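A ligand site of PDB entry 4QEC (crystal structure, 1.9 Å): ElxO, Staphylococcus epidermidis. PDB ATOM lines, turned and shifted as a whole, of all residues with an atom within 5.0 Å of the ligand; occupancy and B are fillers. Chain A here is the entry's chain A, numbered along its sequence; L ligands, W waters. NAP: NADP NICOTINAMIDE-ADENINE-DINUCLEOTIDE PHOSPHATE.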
ATOM      1  N   THR A   8       5.744 -34.694   8.727  1.00  0.00           N
ATOM      2  CA  THR A   8       5.218 -34.705   7.368  1.00  0.00           C
ATOM      3  C   THR A   8       5.459 -33.314   6.757  1.00  0.00           C
ATOM      4  O   THR A   8       4.695 -32.388   6.962  1.00  0.00           O
ATOM      5  CB  THR A   8       3.738 -35.134   7.325  1.00  0.00           C
ATOM      6  OG1 THR A   8       2.933 -34.262   8.126  1.00  0.00           O
ATOM      7  CG2 THR A   8       3.609 -36.587   7.861  1.00  0.00           C
ATOM      8  N   GLY A   9       6.559 -33.199   6.030  1.00  0.00           N
ATOM      9  CA  GLY A   9       7.045 -31.909   5.554  1.00  0.00           C
ATOM     10  C   GLY A   9       8.431 -31.703   6.098  1.00  0.00           C
ATOM     11  O   GLY A   9       9.105 -32.672   6.502  1.00  0.00           O
ATOM     12  N   GLY A  10       8.865 -30.457   6.131  1.00  0.00           N
ATOM     13  CA  GLY A  10      10.182 -30.113   6.643  1.00  0.00           C
ATOM     14  C   GLY A  10      10.972 -29.203   5.726  1.00  0.00           C
ATOM     15  O   GLY A  10      12.055 -28.749   6.101  1.00  0.00           O
ATOM     16  N   PHE A  11      10.458 -28.941   4.539  1.00  0.00           N
ATOM     17  CA  PHE A  11      11.254 -28.176   3.563  1.00  0.00           C
ATOM     18  C   PHE A  11      10.886 -26.704   3.482  1.00  0.00           C
ATOM     19  O   PHE A  11      11.631 -25.912   2.910  1.00  0.00           O
ATOM     20  CB  PHE A  11      11.243 -28.847   2.173  1.00  0.00           C
ATOM     21  CG  PHE A  11      12.130 -30.064   2.107  1.00  0.00           C
ATOM     22  CD1 PHE A  11      11.618 -31.329   2.411  1.00  0.00           C
ATOM     23  CD2 PHE A  11      13.470 -29.959   1.749  1.00  0.00           C
ATOM     24  CE1 PHE A  11      12.429 -32.452   2.358  1.00  0.00           C
ATOM     25  CE2 PHE A  11      14.292 -31.073   1.693  1.00  0.00           C
ATOM     26  CZ  PHE A  11      13.771 -32.324   2.000  1.00  0.00           C
ATOM     27  N   LYS A  12       9.747 -26.323   4.065  1.00  0.00           N
ATOM     28  CA  LYS A  12       9.310 -24.930   4.035  1.00  0.00           C
ATOM     29  C   LYS A  12       8.400 -24.646   5.226  1.00  0.00           C
ATOM     30  O   LYS A  12       7.968 -25.579   5.912  1.00  0.00           O
ATOM     31  CB  LYS A  12       8.558 -24.616   2.729  1.00  0.00           C
ATOM     32  CG  LYS A  12       7.330 -25.478   2.476  1.00  0.00           C
ATOM     33  CD  LYS A  12       6.372 -24.830   1.481  1.00  0.00           C
ATOM     34  CE  LYS A  12       6.681 -25.234   0.054  1.00  0.00           C
ATOM     35  NZ  LYS A  12       5.596 -24.755  -0.856  1.00  0.00           N
ATOM     36  N   GLY A  13       8.097 -23.371   5.447  1.00  0.00           N
ATOM     37  CA  GLY A  13       7.146 -22.955   6.475  1.00  0.00           C
ATOM     38  C   GLY A  13       7.385 -23.532   7.852  1.00  0.00           C
ATOM     39  O   GLY A  13       8.527 -23.722   8.268  1.00  0.00           O
ATOM     40  N   ILE A  14       6.288 -23.836   8.544  1.00  0.00           N
ATOM     41  CA  ILE A  14       6.331 -24.324   9.921  1.00  0.00           C
ATOM     42  C   ILE A  14       7.170 -25.602  10.033  1.00  0.00           C
ATOM     43  O   ILE A  14       7.997 -25.720  10.930  1.00  0.00           O
ATOM     44  CB  ILE A  14       4.898 -24.518  10.481  1.00  0.00           C
ATOM     45  CG1 ILE A  14       4.231 -23.149  10.680  1.00  0.00           C
ATOM     46  CG2 ILE A  14       4.908 -25.310  11.793  1.00  0.00           C
ATOM     47  CD1 ILE A  14       2.707 -23.179  10.739  1.00  0.00           C
ATOM     48  N   GLY A  15       6.979 -26.519   9.085  1.00  0.00           N
ATOM     49  CA  GLY A  15       7.676 -27.813   9.074  1.00  0.00           C
ATOM     50  C   GLY A  15       9.187 -27.726   9.098  1.00  0.00           C
ATOM     51  O   GLY A  15       9.839 -28.502   9.795  1.00  0.00           O
ATOM     52  N   THR A  32       9.996 -35.096   4.960  1.00  0.00           N
ATOM     53  CA  THR A  32       9.357 -35.607   3.751  1.00  0.00           C
ATOM     54  C   THR A  32       8.967 -34.495   2.795  1.00  0.00           C
ATOM     55  O   THR A  32       8.773 -33.339   3.198  1.00  0.00           O
ATOM     56  CB  THR A  32       8.094 -36.498   4.057  1.00  0.00           C
ATOM     57  OG1 THR A  32       6.964 -35.677   4.359  1.00  0.00           O
ATOM     58  CG2 THR A  32       8.345 -37.516   5.206  1.00  0.00           C
ATOM     59  N   SER A  33       8.844 -34.865   1.522  1.00  0.00           N
ATOM     60  CA  SER A  33       8.240 -34.024   0.508  1.00  0.00           C
ATOM     61  C   SER A  33       7.560 -34.957  -0.499  1.00  0.00           C
ATOM     62  O   SER A  33       7.921 -36.129  -0.603  1.00  0.00           O
ATOM     63  CB  SER A  33       9.291 -33.192  -0.208  1.00  0.00           C
ATOM     64  OG  SER A  33       8.716 -32.466  -1.283  1.00  0.00           O
ATOM     65  N   ARG A  34       6.583 -34.435  -1.223  1.00  0.00           N
ATOM     66  CA  ARG A  34       6.005 -35.167  -2.345  1.00  0.00           C
ATOM     67  C   ARG A  34       6.987 -35.239  -3.510  1.00  0.00           C
ATOM     68  O   ARG A  34       6.847 -36.069  -4.412  1.00  0.00           O
ATOM     69  CB  ARG A  34       4.718 -34.472  -2.824  1.00  0.00           C
ATOM     70  CG  ARG A  34       3.567 -34.587  -1.827  1.00  0.00           C
ATOM     71  CD  ARG A  34       2.456 -33.603  -2.158  1.00  0.00           C
ATOM     72  NE  ARG A  34       2.864 -32.225  -1.947  1.00  0.00           N
ATOM     73  CZ  ARG A  34       2.069 -31.172  -2.152  1.00  0.00           C
ATOM     74  NH1 ARG A  34       0.814 -31.361  -2.575  1.00  0.00           N
ATOM     75  NH2 ARG A  34       2.527 -29.949  -1.947  1.00  0.00           N
ATOM     76  N   TYR A  35       7.991 -34.355  -3.473  1.00  0.00           N
ATOM     77  CA  TYR A  35       8.905 -34.157  -4.593  1.00  0.00           C
ATOM     78  C   TYR A  35      10.272 -34.703  -4.247  1.00  0.00           C
ATOM     79  O   TYR A  35      10.922 -34.218  -3.319  1.00  0.00           O
ATOM     80  CB  TYR A  35       8.963 -32.659  -4.952  1.00  0.00           C
ATOM     81  CG  TYR A  35       7.604 -32.108  -5.266  1.00  0.00           C
ATOM     82  CD1 TYR A  35       7.063 -32.241  -6.537  1.00  0.00           C
ATOM     83  CD2 TYR A  35       6.829 -31.493  -4.280  1.00  0.00           C
ATOM     84  CE1 TYR A  35       5.799 -31.762  -6.842  1.00  0.00           C
ATOM     85  CE2 TYR A  35       5.564 -31.000  -4.558  1.00  0.00           C
ATOM     86  CZ  TYR A  35       5.054 -31.144  -5.845  1.00  0.00           C
ATOM     87  OH  TYR A  35       3.802 -30.663  -6.162  1.00  0.00           O
ATOM     88  N   LYS A  38      13.590 -32.515  -3.882  1.00  0.00           N
ATOM     89  CA  LYS A  38      13.898 -31.706  -2.711  1.00  0.00           C
ATOM     90  C   LYS A  38      15.012 -32.282  -1.850  1.00  0.00           C
ATOM     91  O   LYS A  38      15.660 -31.551  -1.099  1.00  0.00           O
ATOM     92  CB  LYS A  38      12.636 -31.402  -1.889  1.00  0.00           C
ATOM     93  CG  LYS A  38      11.652 -30.476  -2.602  1.00  0.00           C
ATOM     94  CD  LYS A  38      10.716 -29.744  -1.642  1.00  0.00           C
ATOM     95  CE  LYS A  38       9.625 -28.992  -2.403  1.00  0.00           C
ATOM     96  NZ  LYS A  38       8.660 -28.309  -1.497  1.00  0.00           N
ATOM     97  N   LEU A  58       6.949 -38.775   0.160  1.00  0.00           N
ATOM     98  CA  LEU A  58       5.672 -39.183   0.751  1.00  0.00           C
ATOM     99  C   LEU A  58       4.543 -38.209   0.380  1.00  0.00           C
ATOM    100  O   LEU A  58       4.684 -36.990   0.538  1.00  0.00           O
ATOM    101  CB  LEU A  58       5.786 -39.291   2.280  1.00  0.00           C
ATOM    102  CG  LEU A  58       4.490 -39.608   3.060  1.00  0.00           C
ATOM    103  CD1 LEU A  58       3.951 -40.991   2.733  1.00  0.00           C
ATOM    104  CD2 LEU A  58       4.702 -39.454   4.566  1.00  0.00           C
ATOM    105  N   ASP A  59       3.444 -38.763  -0.124  1.00  0.00           N
ATOM    106  CA  ASP A  59       2.199 -38.020  -0.206  1.00  0.00           C
ATOM    107  C   ASP A  59       1.295 -38.601   0.882  1.00  0.00           C
ATOM    108  O   ASP A  59       0.976 -39.788   0.834  1.00  0.00           O
ATOM    109  CB  ASP A  59       1.564 -38.191  -1.587  1.00  0.00           C
ATOM    110  CG  ASP A  59       0.439 -37.191  -1.847  1.00  0.00           C
ATOM    111  OD1 ASP A  59      -0.434 -36.994  -0.959  1.00  0.00           O
ATOM    112  OD2 ASP A  59       0.440 -36.586  -2.933  1.00  0.00           O
ATOM    113  N   VAL A  60       0.887 -37.762   1.844  1.00  0.00           N
ATOM    114  CA  VAL A  60       0.076 -38.249   2.976  1.00  0.00           C
ATOM    115  C   VAL A  60      -1.339 -38.704   2.598  1.00  0.00           C
ATOM    116  O   VAL A  60      -2.004 -39.374   3.393  1.00  0.00           O
ATOM    117  CB  VAL A  60       0.012 -37.242   4.171  1.00  0.00           C
ATOM    118  CG1 VAL A  60       1.378 -37.068   4.823  1.00  0.00           C
ATOM    119  CG2 VAL A  60      -0.589 -35.902   3.753  1.00  0.00           C
ATOM    120  N   THR A  61      -1.797 -38.379   1.391  1.00  0.00           N
ATOM    121  CA  THR A  61      -3.114 -38.834   0.926  1.00  0.00           C
ATOM    122  C   THR A  61      -3.076 -40.266   0.380  1.00  0.00           C
ATOM    123  O   THR A  61      -4.123 -40.854   0.079  1.00  0.00           O
ATOM    124  CB  THR A  61      -3.696 -37.892  -0.152  1.00  0.00           C
ATOM    125  OG1 THR A  61      -2.894 -37.967  -1.335  1.00  0.00           O
ATOM    126  CG2 THR A  61      -3.720 -36.448   0.355  1.00  0.00           C
ATOM    127  N   ASN A  86       2.370 -32.267  10.163  1.00  0.00           N
ATOM    128  CA  ASN A  86       2.531 -30.900   9.664  1.00  0.00           C
ATOM    129  C   ASN A  86       1.828 -30.639   8.332  1.00  0.00           C
ATOM    130  O   ASN A  86       1.254 -29.573   8.130  1.00  0.00           O
ATOM    131  CB  ASN A  86       4.027 -30.565   9.553  1.00  0.00           C
ATOM    132  CG  ASN A  86       4.283 -29.245   8.834  1.00  0.00           C
ATOM    133  OD1 ASN A  86       4.658 -29.226   7.659  1.00  0.00           O
ATOM    134  ND2 ASN A  86       4.072 -28.143   9.538  1.00  0.00           N
ATOM    135  N   ALA A  87       1.891 -31.620   7.419  1.00  0.00           N
ATOM    136  CA  ALA A  87       1.322 -31.485   6.070  1.00  0.00           C
ATOM    137  C   ALA A  87      -0.118 -30.991   6.101  1.00  0.00           C
ATOM    138  O   ALA A  87      -0.969 -31.572   6.771  1.00  0.00           O
ATOM    139  CB  ALA A  87       1.391 -32.816   5.334  1.00  0.00           C
ATOM    140  N   GLY A  88      -0.378 -29.891   5.384  1.00  0.00           N
ATOM    141  CA  GLY A  88      -1.716 -29.335   5.319  1.00  0.00           C
ATOM    142  C   GLY A  88      -1.809 -28.271   4.243  1.00  0.00           C
ATOM    143  O   GLY A  88      -0.799 -27.634   3.903  1.00  0.00           O
ATOM    144  N   ILE A  89      -3.023 -28.079   3.731  1.00  0.00           N
ATOM    145  CA  ILE A  89      -3.273 -27.104   2.673  1.00  0.00           C
ATOM    146  C   ILE A  89      -4.492 -26.237   2.980  1.00  0.00           C
ATOM    147  O   ILE A  89      -5.427 -26.663   3.688  1.00  0.00           O
ATOM    148  CB  ILE A  89      -3.466 -27.777   1.287  1.00  0.00           C
ATOM    149  CG1 ILE A  89      -4.514 -28.884   1.379  1.00  0.00           C
ATOM    150  CG2 ILE A  89      -2.140 -28.316   0.764  1.00  0.00           C
ATOM    151  CD1 ILE A  89      -4.984 -29.422   0.044  1.00  0.00           C
ATOM    152  N   THR A 110      -6.006 -34.167   2.409  1.00  0.00           N
ATOM    153  CA  THR A 110      -4.707 -33.852   2.993  1.00  0.00           C
ATOM    154  C   THR A 110      -4.783 -33.630   4.506  1.00  0.00           C
ATOM    155  O   THR A 110      -4.036 -34.239   5.278  1.00  0.00           O
ATOM    156  CB  THR A 110      -4.069 -32.621   2.328  1.00  0.00           C
ATOM    157  OG1 THR A 110      -3.932 -32.862   0.919  1.00  0.00           O
ATOM    158  CG2 THR A 110      -2.683 -32.351   2.929  1.00  0.00           C
ATOM    159  N   ILE A 137      -1.320 -30.518  13.812  1.00  0.00           N
ATOM    160  CA  ILE A 137      -1.451 -29.075  13.633  1.00  0.00           C
ATOM    161  C   ILE A 137      -2.873 -28.725  13.208  1.00  0.00           C
ATOM    162  O   ILE A 137      -3.311 -29.079  12.117  1.00  0.00           O
ATOM    163  CB  ILE A 137      -0.387 -28.456  12.714  1.00  0.00           C
ATOM    164  CG1 ILE A 137       1.018 -28.862  13.202  1.00  0.00           C
ATOM    165  CG2 ILE A 137      -0.533 -26.933  12.661  1.00  0.00           C
ATOM    166  CD1 ILE A 137       2.143 -28.298  12.361  1.00  0.00           C
ATOM    167  N   SER A 138      -3.587 -28.048  14.107  1.00  0.00           N
ATOM    168  CA  SER A 138      -4.907 -27.508  13.800  1.00  0.00           C
ATOM    169  C   SER A 138      -4.748 -26.040  13.405  1.00  0.00           C
ATOM    170  O   SER A 138      -3.853 -25.703  12.630  1.00  0.00           O
ATOM    171  CB  SER A 138      -5.838 -27.689  15.013  1.00  0.00           C
ATOM    172  OG  SER A 138      -7.154 -27.235  14.719  1.00  0.00           O
ATOM    173  N   SER A 139      -5.583 -25.159  13.961  1.00  0.00           N
ATOM    174  CA  SER A 139      -5.572 -23.734  13.628  1.00  0.00           C
ATOM    175  C   SER A 139      -6.540 -23.036  14.582  1.00  0.00           C
ATOM    176  O   SER A 139      -7.392 -23.703  15.196  1.00  0.00           O
ATOM    177  CB  SER A 139      -6.038 -23.531  12.168  1.00  0.00           C
ATOM    178  OG  SER A 139      -6.481 -22.215  11.906  1.00  0.00           O
ATOM    179  N   TYR A 152     -11.668 -24.852   5.321  1.00  0.00           N
ATOM    180  CA  TYR A 152     -10.398 -25.124   5.970  1.00  0.00           C
ATOM    181  C   TYR A 152     -10.619 -25.329   7.467  1.00  0.00           C
ATOM    182  O   TYR A 152     -10.088 -26.284   8.039  1.00  0.00           O
ATOM    183  CB  TYR A 152      -9.426 -23.976   5.728  1.00  0.00           C
ATOM    184  CG  TYR A 152      -8.126 -24.073   6.499  1.00  0.00           C
ATOM    185  CD1 TYR A 152      -7.088 -24.919   6.070  1.00  0.00           C
ATOM    186  CD2 TYR A 152      -7.917 -23.286   7.632  1.00  0.00           C
ATOM    187  CE1 TYR A 152      -5.880 -24.994   6.758  1.00  0.00           C
ATOM    188  CE2 TYR A 152      -6.711 -23.361   8.341  1.00  0.00           C
ATOM    189  CZ  TYR A 152      -5.713 -24.209   7.901  1.00  0.00           C
ATOM    190  OH  TYR A 152      -4.524 -24.261   8.586  1.00  0.00           O
ATOM    191  N   LYS A 156      -9.831 -28.452  10.147  1.00  0.00           N
ATOM    192  CA  LYS A 156      -9.028 -28.239  11.342  1.00  0.00           C
ATOM    193  C   LYS A 156      -9.794 -28.571  12.644  1.00  0.00           C
ATOM    194  O   LYS A 156      -9.182 -28.956  13.640  1.00  0.00           O
ATOM    195  CB  LYS A 156      -8.403 -26.838  11.357  1.00  0.00           C
ATOM    196  CG  LYS A 156      -7.359 -26.603  10.269  1.00  0.00           C
ATOM    197  CD  LYS A 156      -6.346 -27.743  10.201  1.00  0.00           C
ATOM    198  CE  LYS A 156      -5.079 -27.360   9.452  1.00  0.00           C
ATOM    199  NZ  LYS A 156      -3.975 -28.375   9.595  1.00  0.00           N
ATOM    200  N   PRO A 182      -2.389 -22.731  15.691  1.00  0.00           N
ATOM    201  CA  PRO A 182      -1.720 -21.452  15.444  1.00  0.00           C
ATOM    202  C   PRO A 182      -2.669 -20.371  14.922  1.00  0.00           C
ATOM    203  O   PRO A 182      -3.650 -20.691  14.241  1.00  0.00           O
ATOM    204  CB  PRO A 182      -0.681 -21.803  14.364  1.00  0.00           C
ATOM    205  CG  PRO A 182      -0.524 -23.281  14.438  1.00  0.00           C
ATOM    206  CD  PRO A 182      -1.917 -23.778  14.776  1.00  0.00           C
ATOM    207  N   GLY A 183      -2.380 -19.121  15.252  1.00  0.00           N
ATOM    208  CA  GLY A 183      -3.001 -17.980  14.565  1.00  0.00           C
ATOM    209  C   GLY A 183      -2.301 -17.783  13.231  1.00  0.00           C
ATOM    210  O   GLY A 183      -1.751 -18.741  12.669  1.00  0.00           O
ATOM    211  N   ILE A 184      -2.316 -16.554  12.695  1.00  0.00           N
ATOM    212  CA  ILE A 184      -1.686 -16.312  11.390  1.00  0.00           C
ATOM    213  C   ILE A 184      -0.165 -16.232  11.531  1.00  0.00           C
ATOM    214  O   ILE A 184       0.378 -15.400  12.280  1.00  0.00           O
ATOM    215  CB  ILE A 184      -2.249 -15.067  10.672  1.00  0.00           C
ATOM    216  CG1 ILE A 184      -3.772 -15.164  10.540  1.00  0.00           C
ATOM    217  CG2 ILE A 184      -1.609 -14.926   9.286  1.00  0.00           C
ATOM    218  CD1 ILE A 184      -4.407 -14.005   9.797  1.00  0.00           C
ATOM    219  N   ILE A 185       0.510 -17.134  10.820  1.00  0.00           N
ATOM    220  CA  ILE A 185       1.947 -17.318  10.941  1.00  0.00           C
ATOM    221  C   ILE A 185       2.660 -16.743   9.722  1.00  0.00           C
ATOM    222  O   ILE A 185       2.272 -17.008   8.574  1.00  0.00           O
ATOM    223  CB  ILE A 185       2.303 -18.828  11.144  1.00  0.00           C
ATOM    224  CG1 ILE A 185       1.558 -19.442  12.348  1.00  0.00           C
ATOM    225  CG2 ILE A 185       3.821 -19.022  11.239  1.00  0.00           C
ATOM    226  CD1 ILE A 185       1.668 -18.712  13.676  1.00  0.00           C
ATOM    227  N   THR A 187       4.954 -17.239   7.392  1.00  0.00           N
ATOM    228  CA  THR A 187       5.791 -18.166   6.645  1.00  0.00           C
ATOM    229  C   THR A 187       6.402 -17.449   5.436  1.00  0.00           C
ATOM    230  O   THR A 187       6.089 -16.275   5.189  1.00  0.00           O
ATOM    231  CB  THR A 187       4.977 -19.356   6.133  1.00  0.00           C
ATOM    232  OG1 THR A 187       3.904 -18.866   5.331  1.00  0.00           O
ATOM    233  CG2 THR A 187       4.423 -20.175   7.308  1.00  0.00           C
ATOM    234  N   GLU A 188       7.242 -18.161   4.688  1.00  0.00           N
ATOM    235  CA  GLU A 188       7.794 -17.662   3.423  1.00  0.00           C
ATOM    236  C   GLU A 188       6.689 -17.251   2.446  1.00  0.00           C
ATOM    237  O   GLU A 188       6.762 -16.191   1.823  1.00  0.00           O
ATOM    238  CB  GLU A 188       8.719 -18.695   2.749  1.00  0.00           C
ATOM    239  CG  GLU A 188       9.824 -19.239   3.626  1.00  0.00           C
ATOM    240  CD  GLU A 188       9.515 -20.617   4.204  1.00  0.00           C
ATOM    241  OE1 GLU A 188       8.360 -21.064   4.106  1.00  0.00           O
ATOM    242  OE2 GLU A 188      10.449 -21.258   4.740  1.00  0.00           O
ATOM    243  N   THR A 189       5.652 -18.086   2.346  1.00  0.00           N
ATOM    244  CA  THR A 189       4.521 -17.822   1.470  1.00  0.00           C
ATOM    245  C   THR A 189       3.820 -16.502   1.808  1.00  0.00           C
ATOM    246  O   THR A 189       3.536 -15.709   0.914  1.00  0.00           O
ATOM    247  CB  THR A 189       3.514 -19.001   1.500  1.00  0.00           C
ATOM    248  OG1 THR A 189       4.199 -20.217   1.185  1.00  0.00           O
ATOM    249  CG2 THR A 189       2.391 -18.778   0.487  1.00  0.00           C
HETATM  250  PA  NAP L   1       3.403 -24.585   3.767  1.00  0.00           P
HETATM  251  O1A NAP L   1       4.542 -23.648   4.056  1.00  0.00           O
HETATM  252  O2A NAP L   1       2.449 -24.379   2.646  1.00  0.00           O
HETATM  253  O5B NAP L   1       4.033 -26.054   3.586  1.00  0.00           O
HETATM  254  C5B NAP L   1       3.168 -27.180   3.378  1.00  0.00           C
HETATM  255  C4B NAP L   1       3.915 -28.439   3.782  1.00  0.00           C
HETATM  256  O4B NAP L   1       3.008 -29.549   3.746  1.00  0.00           O
HETATM  257  C3B NAP L   1       5.037 -28.775   2.811  1.00  0.00           C
HETATM  258  O3B NAP L   1       6.097 -29.364   3.574  1.00  0.00           O
HETATM  259  C2B NAP L   1       4.427 -29.796   1.865  1.00  0.00           C
HETATM  260  O2B NAP L   1       5.385 -30.686   1.275  1.00  0.00           O
HETATM  261  C1B NAP L   1       3.466 -30.525   2.791  1.00  0.00           C
HETATM  262  N9A NAP L   1       2.331 -31.150   2.063  1.00  0.00           N
HETATM  263  C8A NAP L   1       1.274 -30.547   1.519  1.00  0.00           C
HETATM  264  N7A NAP L   1       0.478 -31.493   0.957  1.00  0.00           N
HETATM  265  C5A NAP L   1       1.063 -32.689   1.172  1.00  0.00           C
HETATM  266  C6A NAP L   1       0.710 -33.989   0.843  1.00  0.00           C
HETATM  267  N6A NAP L   1      -0.426 -34.232   0.148  1.00  0.00           N
HETATM  268  N1A NAP L   1       1.533 -35.008   1.224  1.00  0.00           N
HETATM  269  C2A NAP L   1       2.669 -34.774   1.901  1.00  0.00           C
HETATM  270  N3A NAP L   1       3.030 -33.524   2.224  1.00  0.00           N
HETATM  271  C4A NAP L   1       2.237 -32.471   1.871  1.00  0.00           C
HETATM  272  O3  NAP L   1       2.511 -24.842   5.079  1.00  0.00           O
HETATM  273  PN  NAP L   1       2.539 -24.047   6.471  1.00  0.00           P
HETATM  274  O1N NAP L   1       3.862 -24.201   7.161  1.00  0.00           O
HETATM  275  O2N NAP L   1       1.891 -22.689   6.291  1.00  0.00           O
HETATM  276  O5D NAP L   1       1.459 -24.942   7.254  1.00  0.00           O
HETATM  277  C5D NAP L   1       1.876 -26.120   7.963  1.00  0.00           C
HETATM  278  C4D NAP L   1       0.695 -26.654   8.763  1.00  0.00           C
HETATM  279  O4D NAP L   1       0.263 -25.637   9.673  1.00  0.00           O
HETATM  280  C3D NAP L   1      -0.520 -26.978   7.880  1.00  0.00           C
HETATM  281  O3D NAP L   1      -1.245 -28.070   8.467  1.00  0.00           O
HETATM  282  C2D NAP L   1      -1.346 -25.710   7.967  1.00  0.00           C
HETATM  283  O2D NAP L   1      -2.725 -25.903   7.598  1.00  0.00           O
HETATM  284  C1D NAP L   1      -1.115 -25.311   9.423  1.00  0.00           C
HETATM  285  N1N NAP L   1      -1.367 -23.898   9.742  1.00  0.00           N
HETATM  286  C2N NAP L   1      -0.732 -22.896   9.075  1.00  0.00           C
HETATM  287  C3N NAP L   1      -1.003 -21.575   9.432  1.00  0.00           C
HETATM  288  C7N NAP L   1      -0.356 -20.409   8.734  1.00  0.00           C
HETATM  289  O7N NAP L   1      -0.660 -19.292   9.108  1.00  0.00           O
HETATM  290  N7N NAP L   1       0.535 -20.606   7.744  1.00  0.00           N
HETATM  291  C4N NAP L   1      -1.913 -21.305  10.471  1.00  0.00           C
HETATM  292  C5N NAP L   1      -2.531 -22.361  11.146  1.00  0.00           C
HETATM  293  C6N NAP L   1      -2.217 -23.659  10.756  1.00  0.00           C
HETATM  294  P2B NAP L   1       5.853 -30.615  -0.276  1.00  0.00           P
HETATM  295  O1X NAP L   1       5.177 -29.414  -0.862  1.00  0.00           O
HETATM  296  O2X NAP L   1       7.360 -30.490  -0.181  1.00  0.00           O
HETATM  297  O3X NAP L   1       5.358 -31.912  -0.840  1.00  0.00           O
HETATM  298  O   HOH W   1       6.312 -27.729  -2.759  1.00  0.00           O
HETATM  299  O   HOH W   2       2.124 -20.734   4.559  1.00  0.00           O
HETATM  300  O   HOH W   3       0.175 -17.633   6.915  1.00  0.00           O
HETATM  301  O   HOH W   4       7.483 -28.274   5.564  1.00  0.00           O
HETATM  302  O   HOH W   5      -2.433 -24.858   4.937  1.00  0.00           O
HETATM  303  O   HOH W   6       1.886 -21.811   1.786  1.00  0.00           O
HETATM  304  O   HOH W   7       4.035 -26.978  -0.587  1.00  0.00           O
HETATM  305  O   HOH W   8      -0.781 -22.923   5.213  1.00  0.00           O
HETATM  306  O   HOH W   9       0.140 -25.863   2.132  1.00  0.00           O
HETATM  307  O   HOH W  10       5.104 -26.617   6.790  1.00  0.00           O
HETATM  308  O   HOH W  11       5.670 -21.358   3.082  1.00  0.00           O
HETATM  309  O   HOH W  12       3.021 -23.793  -0.096  1.00  0.00           O
HETATM  310  O   HOH W  13       8.243 -30.499   2.386  1.00  0.00           O
HETATM  311  O   HOH W  14      -1.912 -31.843  -0.478  1.00  0.00           O
HETATM  312  O   HOH W  15      -1.431 -30.833   9.375  1.00  0.00           O
HETATM  313  O   HOH W  16       5.745 -34.696   2.207  1.00  0.00           O
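The backbone NH (N) of Tyr 35 is in hydrogen-bond range of the side-chain hydroxyl (OG) of Ser 33, at 3.0 Å.
O of Ile 137 lies within hydrogen-bond range of NZ of Lys 156, 2.7 Å away.
OD1 of Asp 59 is in hydrogen-bond range of OG1 of Thr 61, 2.7 Å away.
The side-chain hydroxyl (OG) of Ser 138 lies within hydrogen-bond range of the backbone carbonyl oxygen (O) of Lys 156 (2.9 Å).
The side-chain carboxylate (OE1) of Glu 188 lies within hydrogen-bond range of the backbone NH (N) of Gly 13 (2.7 Å).
N of Asn 86 is in hydrogen-bond range of OG1 of Thr 8, 2.9 Å away.
The backbone NH (N) of Ala 87 lies within hydrogen-bond range of the side-chain hydroxyl (OG1) of Thr 8, 2.9 Å away.
ND2 of Asn 86 sits close to N of Gly 15.
Residues that only touch the ligand: Gly 9 (3.4 Å), Gly 10 (3.9 Å), Lys 12 (3.4 Å), Gly 13 (3.6 Å), Tyr 35 (3.8 Å), Leu 58 (3.3 Å), Thr 61 (3.98 Å), Ala 87 (3.5 Å), Gly 88 (3.4 Å), Thr 110 (3.8 Å), Ile 137 (3.4 Å), Ser 138 (3.2 Å), Ser 139 (3.8 Å), Pro 182 (3.7 Å), Gly 183 (3.4 Å), Ile 184 (3.9 Å) and Thr 187 (3.7 Å).
Hydrophobic or aromatic side chains within 4 Å of the ligand: Ile 14, Tyr 35, Val 60, Ala 87, Ile 137, Tyr 152, Pro 182 and Ile 185.
Of the 34 residues printed, 27 come within 4 Å of the ligand.
The nearest printed residue that does not touch the ligand is Ile 89 (4.1 Å).
Water W13 lies within hydrogen-bond range of O3B of the ligand (2.7 Å), O of Thr 32 (3.0 Å) and N of Phe 11 (3.5 Å).
Water W6 bridges O2A of the ligand (2.8 Å) and OG1 of Thr 189 (2.9 Å).
Water W1 bridges NZ of Lys 38 (2.7 Å) and O1X of the ligand (2.8 Å).
Water W12 bridges NZ of Lys 12 (2.9 Å) and O2A of the ligand (2.9 Å).
Water W5 lies within hydrogen-bond range of O2D of the ligand, O of Gly 88 and N of Ile 89.
Water W16 lies within hydrogen-bond range of the side-chain hydroxyl of Thr 32, a nitrogen (N3A) of the ligand, the backbone carbonyl oxygen of Leu 58 and the backbone NH of Ser 33.
O3D of the ligand sits at hydrogen-bond distance from NZ of Lys 156, at 3.0 Å.
An oxygen (O1N) of the ligand lies within hydrogen-bond range of the backbone NH (N) of Ile 14 (2.8 Å).
An oxygen (O2D) of the ligand sits at hydrogen-bond distance from the side-chain hydroxyl (OH) of Tyr 152 (2.6 Å).
OG of Ser 33 is in hydrogen-bond range of O2X of the ligand, 2.6 Å away.
A nitrogen (N1A) of the ligand lies within hydrogen-bond range of the backbone NH (N) of Val 60 (2.9 Å).
The backbone NH (N) of Arg 34 sits at hydrogen-bond distance from an oxygen (O3X) of the ligand (2.8 Å).
NE of Arg 34 is in salt-bridge range of O3X of the ligand, at 2.7 Å.
The side-chain amino group (NZ) of Lys 38 is in salt-bridge range of an oxygen (O2X) of the ligand (2.9 Å).
O of Asn 86 is in hydrogen-bond range of O3D of the ligand (2.9 Å).
OD1 of Asp 59 is in hydrogen-bond range of N6A of the ligand, at 3.0 Å.
The backbone NH (N) of Ile 185 is in hydrogen-bond range of an oxygen (O7N) of the ligand, at 3.0 Å.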
